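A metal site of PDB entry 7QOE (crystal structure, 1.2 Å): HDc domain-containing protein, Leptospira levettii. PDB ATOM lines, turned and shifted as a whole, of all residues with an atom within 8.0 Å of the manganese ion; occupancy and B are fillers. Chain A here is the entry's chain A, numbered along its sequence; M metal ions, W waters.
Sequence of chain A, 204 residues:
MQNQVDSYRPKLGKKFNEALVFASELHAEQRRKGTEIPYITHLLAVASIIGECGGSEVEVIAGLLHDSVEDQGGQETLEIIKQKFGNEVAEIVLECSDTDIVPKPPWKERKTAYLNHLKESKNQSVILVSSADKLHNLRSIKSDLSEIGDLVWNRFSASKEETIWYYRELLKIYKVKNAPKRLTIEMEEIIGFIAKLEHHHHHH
The manganese ion is bound by water W2 (2.1 Å), a ring nitrogen (NE2) of His 66 (2.1 Å), water W1 (2.1 Å), a ring nitrogen (NE2) of His 42 (2.2 Å), the side-chain carboxylate (OD2) of Asp 133 (2.2 Å) and the side-chain carboxylate (OD1) of Asp 67 (2.3 Å). The manganese ion has six donor atoms within binding distance.
Residues that only touch the manganese ion: Tyr 39 (3.8 Å). Along chain A the residues within 4 Å of the manganese ion span positions 39 to 133.
Water W2 bridges the side-chain hydroxyl (OH) of Tyr 39 and the side-chain amide nitrogen (ND2) of Asn 137. Water W1 bridges OD2 of Asp 67 (2.6 Å) and OD1 of Asp 133 (2.6 Å).
ND1 of His 136 sits at hydrogen-bond distance from ND1 of His 42. The backbone carbonyl oxygen of Gly 63 is in hydrogen-bond range of a ring nitrogen (ND1) of His 66 (2.8 Å). The side-chain hydroxyl of Tyr 39 lies close to the side-chain carboxylate of Asp 67 (2.6 Å). The backbone carbonyl oxygen of Asp 133 sits close to the side-chain amide nitrogen of Asn 137 (3.4 Å). The side-chain carboxylate (OD1) of Asp 133 lies within salt-bridge range of the side-chain amino group (NZ) of Lys 134.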
ATOM      1  N   ARG A  32     -12.676  -2.410  15.724  1.00  0.00           N
ATOM      2  CA  ARG A  32     -13.424  -2.295  14.475  1.00  0.00           C
ATOM      3  C   ARG A  32     -14.294  -1.052  14.578  1.00  0.00           C
ATOM      4  O   ARG A  32     -14.916  -0.788  15.619  1.00  0.00           O
ATOM      5  CB  ARG A  32     -14.263  -3.545  14.294  1.00  0.00           C
ATOM      6  CG  ARG A  32     -13.446  -4.857  14.376  1.00  0.00           C
ATOM      7  CD  ARG A  32     -12.643  -5.120  13.124  1.00  0.00           C
ATOM      8  NE  ARG A  32     -13.524  -5.492  12.018  1.00  0.00           N
ATOM      9  CZ  ARG A  32     -14.045  -6.708  11.842  1.00  0.00           C
ATOM     10  NH1 ARG A  32     -13.703  -7.739  12.611  1.00  0.00           N
ATOM     11  NH2 ARG A  32     -14.933  -6.888  10.868  1.00  0.00           N
ATOM     12  N   TYR A  39      -9.654  -5.109  16.923  1.00  0.00           N
ATOM     13  CA  TYR A  39      -9.320  -5.103  15.498  1.00  0.00           C
ATOM     14  C   TYR A  39      -8.585  -6.365  15.059  1.00  0.00           C
ATOM     15  O   TYR A  39      -8.647  -6.747  13.879  1.00  0.00           O
ATOM     16  CB  TYR A  39      -8.470  -3.874  15.174  1.00  0.00           C
ATOM     17  CG  TYR A  39      -8.480  -3.555  13.693  1.00  0.00           C
ATOM     18  CD1 TYR A  39      -9.585  -2.928  13.123  1.00  0.00           C
ATOM     19  CD2 TYR A  39      -7.421  -3.876  12.865  1.00  0.00           C
ATOM     20  CE1 TYR A  39      -9.622  -2.631  11.774  1.00  0.00           C
ATOM     21  CE2 TYR A  39      -7.454  -3.592  11.499  1.00  0.00           C
ATOM     22  CZ  TYR A  39      -8.566  -2.968  10.964  1.00  0.00           C
ATOM     23  OH  TYR A  39      -8.668  -2.649   9.626  1.00  0.00           O
ATOM     24  N   HIS A  42     -10.178  -8.859  12.646  1.00  0.00           N
ATOM     25  CA  HIS A  42     -10.162  -8.662  11.196  1.00  0.00           C
ATOM     26  C   HIS A  42      -8.887  -9.257  10.604  1.00  0.00           C
ATOM     27  O   HIS A  42      -8.928  -9.920   9.570  1.00  0.00           O
ATOM     28  CB  HIS A  42     -10.295  -7.158  10.864  1.00  0.00           C
ATOM     29  CG  HIS A  42      -9.868  -6.790   9.475  1.00  0.00           C
ATOM     30  ND1 HIS A  42     -10.608  -7.130   8.361  1.00  0.00           N
ATOM     31  CD2 HIS A  42      -8.859  -5.987   9.029  1.00  0.00           C
ATOM     32  CE1 HIS A  42     -10.030  -6.619   7.280  1.00  0.00           C
ATOM     33  NE2 HIS A  42      -8.983  -5.915   7.654  1.00  0.00           N
ATOM     34  N   LEU A  43      -7.752  -8.992  11.236  1.00  0.00           N
ATOM     35  CA  LEU A  43      -6.475  -9.449  10.726  1.00  0.00           C
ATOM     36  C   LEU A  43      -6.363 -10.963  10.743  1.00  0.00           C
ATOM     37  O   LEU A  43      -5.859 -11.566   9.780  1.00  0.00           O
ATOM     38  CB  LEU A  43      -5.357  -8.789  11.536  1.00  0.00           C
ATOM     39  CG  LEU A  43      -5.370  -7.246  11.522  1.00  0.00           C
ATOM     40  CD1 LEU A  43      -4.301  -6.635  12.434  1.00  0.00           C
ATOM     41  CD2 LEU A  43      -5.271  -6.714  10.087  1.00  0.00           C
ATOM     42  N   VAL A  46      -8.522 -12.277   7.820  1.00  0.00           N
ATOM     43  CA  VAL A  46      -7.884 -12.077   6.517  1.00  0.00           C
ATOM     44  C   VAL A  46      -6.747 -13.066   6.344  1.00  0.00           C
ATOM     45  O   VAL A  46      -6.610 -13.683   5.270  1.00  0.00           O
ATOM     46  CB  VAL A  46      -7.426 -10.617   6.406  1.00  0.00           C
ATOM     47  CG1 VAL A  46      -6.507 -10.427   5.205  1.00  0.00           C
ATOM     48  CG2 VAL A  46      -8.620  -9.679   6.333  1.00  0.00           C
ATOM     49  N   GLY A  63      -1.010 -10.443   5.079  1.00  0.00           N
ATOM     50  CA  GLY A  63      -2.412 -10.291   5.456  1.00  0.00           C
ATOM     51  C   GLY A  63      -2.579  -9.857   6.894  1.00  0.00           C
ATOM     52  O   GLY A  63      -3.404  -8.995   7.201  1.00  0.00           O
ATOM     53  N   LEU A  65      -0.602  -8.079   8.516  1.00  0.00           N
ATOM     54  CA  LEU A  65       0.006  -6.772   8.673  1.00  0.00           C
ATOM     55  C   LEU A  65      -0.507  -5.736   7.673  1.00  0.00           C
ATOM     56  O   LEU A  65       0.026  -4.620   7.631  1.00  0.00           O
ATOM     57  CB  LEU A  65       1.532  -6.893   8.569  1.00  0.00           C
ATOM     58  CG  LEU A  65       2.161  -7.870   9.557  1.00  0.00           C
ATOM     59  CD1 LEU A  65       3.659  -7.918   9.403  1.00  0.00           C
ATOM     60  CD2 LEU A  65       1.804  -7.516  10.991  1.00  0.00           C
ATOM     61  N   HIS A  66      -1.556  -6.041   6.912  1.00  0.00           N
ATOM     62  CA  HIS A  66      -1.908  -5.183   5.790  1.00  0.00           C
ATOM     63  C   HIS A  66      -2.431  -3.820   6.239  1.00  0.00           C
ATOM     64  O   HIS A  66      -2.416  -2.886   5.431  1.00  0.00           O
ATOM     65  CB  HIS A  66      -2.898  -5.882   4.852  1.00  0.00           C
ATOM     66  CG  HIS A  66      -4.300  -5.865   5.351  1.00  0.00           C
ATOM     67  ND1 HIS A  66      -4.790  -6.831   6.199  1.00  0.00           N
ATOM     68  CD2 HIS A  66      -5.308  -4.995   5.138  1.00  0.00           C
ATOM     69  CE1 HIS A  66      -6.045  -6.546   6.503  1.00  0.00           C
ATOM     70  NE2 HIS A  66      -6.385  -5.436   5.869  1.00  0.00           N
ATOM     71  N   ASP A  67      -2.911  -3.685   7.480  1.00  0.00           N
ATOM     72  CA  ASP A  67      -3.390  -2.400   7.992  1.00  0.00           C
ATOM     73  C   ASP A  67      -2.399  -1.738   8.958  1.00  0.00           C
ATOM     74  O   ASP A  67      -2.709  -0.690   9.530  1.00  0.00           O
ATOM     75  CB  ASP A  67      -4.763  -2.557   8.647  1.00  0.00           C
ATOM     76  CG  ASP A  67      -5.879  -2.736   7.622  1.00  0.00           C
ATOM     77  OD1 ASP A  67      -6.859  -3.474   7.881  1.00  0.00           O
ATOM     78  OD2 ASP A  67      -5.753  -2.160   6.518  1.00  0.00           O
ATOM     79  N   SER A  68      -1.188  -2.284   9.093  1.00  0.00           N
ATOM     80  CA  SER A  68      -0.282  -1.836  10.144  1.00  0.00           C
ATOM     81  C   SER A  68       0.337  -0.485   9.818  1.00  0.00           C
ATOM     82  O   SER A  68       0.602   0.318  10.724  1.00  0.00           O
ATOM     83  CB  SER A  68       0.817  -2.884  10.341  1.00  0.00           C
ATOM     84  OG  SER A  68       1.600  -2.997   9.152  1.00  0.00           O
ATOM     85  N   GLU A  70      -0.975   1.863   7.626  1.00  0.00           N
ATOM     86  CA  GLU A  70      -2.034   2.867   7.602  1.00  0.00           C
ATOM     87  C   GLU A  70      -2.476   3.243   9.009  1.00  0.00           C
ATOM     88  O   GLU A  70      -2.644   4.434   9.322  1.00  0.00           O
ATOM     89  CB  GLU A  70      -3.243   2.323   6.823  1.00  0.00           C
ATOM     90  CG  GLU A  70      -2.987   2.057   5.347  1.00  0.00           C
ATOM     91  CD  GLU A  70      -4.262   2.135   4.528  1.00  0.00           C
ATOM     92  OE1 GLU A  70      -5.369   2.088   5.109  1.00  0.00           O
ATOM     93  OE2 GLU A  70      -4.168   2.238   3.284  1.00  0.00           O
ATOM     94  N   ASP A  71      -2.678   2.249   9.883  1.00  0.00           N
ATOM     95  CA  ASP A  71      -3.357   2.482  11.154  1.00  0.00           C
ATOM     96  C   ASP A  71      -2.435   2.519  12.365  1.00  0.00           C
ATOM     97  O   ASP A  71      -2.860   2.968  13.434  1.00  0.00           O
ATOM     98  CB  ASP A  71      -4.391   1.373  11.420  1.00  0.00           C
ATOM     99  CG  ASP A  71      -5.523   1.367  10.412  1.00  0.00           C
ATOM    100  OD1 ASP A  71      -6.261   0.353  10.377  1.00  0.00           O
ATOM    101  OD2 ASP A  71      -5.707   2.369   9.686  1.00  0.00           O
ATOM    102  N   VAL A 129      -3.990 -10.473  -1.091  1.00  0.00           N
ATOM    103  CA  VAL A 129      -4.195  -9.847   0.215  1.00  0.00           C
ATOM    104  C   VAL A 129      -5.373  -8.886   0.155  1.00  0.00           C
ATOM    105  O   VAL A 129      -6.234  -8.871   1.028  1.00  0.00           O
ATOM    106  CB  VAL A 129      -2.906  -9.142   0.686  1.00  0.00           C
ATOM    107  CG1 VAL A 129      -3.222  -8.283   1.933  1.00  0.00           C
ATOM    108  CG2 VAL A 129      -1.819 -10.162   0.990  1.00  0.00           C
ATOM    109  N   SER A 130      -5.399  -8.041  -0.870  1.00  0.00           N
ATOM    110  CA  SER A 130      -6.469  -7.062  -1.031  1.00  0.00           C
ATOM    111  C   SER A 130      -7.837  -7.731  -1.112  1.00  0.00           C
ATOM    112  O   SER A 130      -8.785  -7.310  -0.431  1.00  0.00           O
ATOM    113  CB  SER A 130      -6.213  -6.215  -2.279  1.00  0.00           C
ATOM    114  OG  SER A 130      -7.197  -5.211  -2.431  1.00  0.00           O
ATOM    115  N   ALA A 132      -8.789 -10.677  -0.062  1.00  0.00           N
ATOM    116  CA  ALA A 132      -9.152 -11.275   1.225  1.00  0.00           C
ATOM    117  C   ALA A 132      -9.634 -10.219   2.214  1.00  0.00           C
ATOM    118  O   ALA A 132     -10.620 -10.444   2.940  1.00  0.00           O
ATOM    119  CB  ALA A 132      -7.952 -12.030   1.798  1.00  0.00           C
ATOM    120  N   ASP A 133      -8.936  -9.098   2.280  1.00  0.00           N
ATOM    121  CA  ASP A 133      -9.342  -7.942   3.099  1.00  0.00           C
ATOM    122  C   ASP A 133     -10.769  -7.515   2.769  1.00  0.00           C
ATOM    123  O   ASP A 133     -11.621  -7.383   3.662  1.00  0.00           O
ATOM    124  CB  ASP A 133      -8.338  -6.834   2.788  1.00  0.00           C
ATOM    125  CG  ASP A 133      -8.543  -5.566   3.554  1.00  0.00           C
ATOM    126  OD1 ASP A 133      -8.023  -4.542   3.032  1.00  0.00           O
ATOM    127  OD2 ASP A 133      -9.131  -5.543   4.656  1.00  0.00           O
ATOM    128  N   LYS A 134     -11.059  -7.325   1.488  1.00  0.00           N
ATOM    129  CA  LYS A 134     -12.369  -6.867   1.082  1.00  0.00           C
ATOM    130  C   LYS A 134     -13.440  -7.917   1.324  1.00  0.00           C
ATOM    131  O   LYS A 134     -14.576  -7.586   1.701  1.00  0.00           O
ATOM    132  CB  LYS A 134     -12.327  -6.457  -0.390  1.00  0.00           C
ATOM    133  CG  LYS A 134     -11.994  -5.003  -0.645  1.00  0.00           C
ATOM    134  CD  LYS A 134     -10.730  -4.539   0.052  1.00  0.00           C
ATOM    135  CE  LYS A 134     -10.531  -3.051  -0.141  1.00  0.00           C
ATOM    136  NZ  LYS A 134      -9.312  -2.514   0.520  1.00  0.00           N
ATOM    137  N   HIS A 136     -13.498 -10.096   3.766  1.00  0.00           N
ATOM    138  CA  HIS A 136     -13.845 -10.043   5.182  1.00  0.00           C
ATOM    139  C   HIS A 136     -14.686  -8.814   5.502  1.00  0.00           C
ATOM    140  O   HIS A 136     -15.653  -8.896   6.268  1.00  0.00           O
ATOM    141  CB  HIS A 136     -12.607 -10.067   6.056  1.00  0.00           C
ATOM    142  CG  HIS A 136     -12.954 -10.080   7.501  1.00  0.00           C
ATOM    143  ND1 HIS A 136     -12.714  -9.015   8.343  1.00  0.00           N
ATOM    144  CD2 HIS A 136     -13.639 -10.987   8.232  1.00  0.00           C
ATOM    145  CE1 HIS A 136     -13.196  -9.290   9.541  1.00  0.00           C
ATOM    146  NE2 HIS A 136     -13.755 -10.487   9.498  1.00  0.00           N
ATOM    147  N   ASN A 137     -14.340  -7.671   4.928  1.00  0.00           N
ATOM    148  CA  ASN A 137     -15.146  -6.475   5.183  1.00  0.00           C
ATOM    149  C   ASN A 137     -16.568  -6.676   4.715  1.00  0.00           C
ATOM    150  O   ASN A 137     -17.519  -6.236   5.385  1.00  0.00           O
ATOM    151  CB  ASN A 137     -14.489  -5.264   4.521  1.00  0.00           C
ATOM    152  CG  ASN A 137     -13.196  -4.873   5.217  1.00  0.00           C
ATOM    153  OD1 ASN A 137     -12.998  -5.176   6.396  1.00  0.00           O
ATOM    154  ND2 ASN A 137     -12.325  -4.205   4.494  1.00  0.00           N
HETATM  155 MN    MN M   1      -8.176  -4.437   6.289  1.00  0.00          MN
HETATM  156  O   HOH W   1      -7.745  -2.834   4.990  1.00  0.00           O
HETATM  157  O   HOH W   2      -9.861  -3.303   6.570  1.00  0.00           O
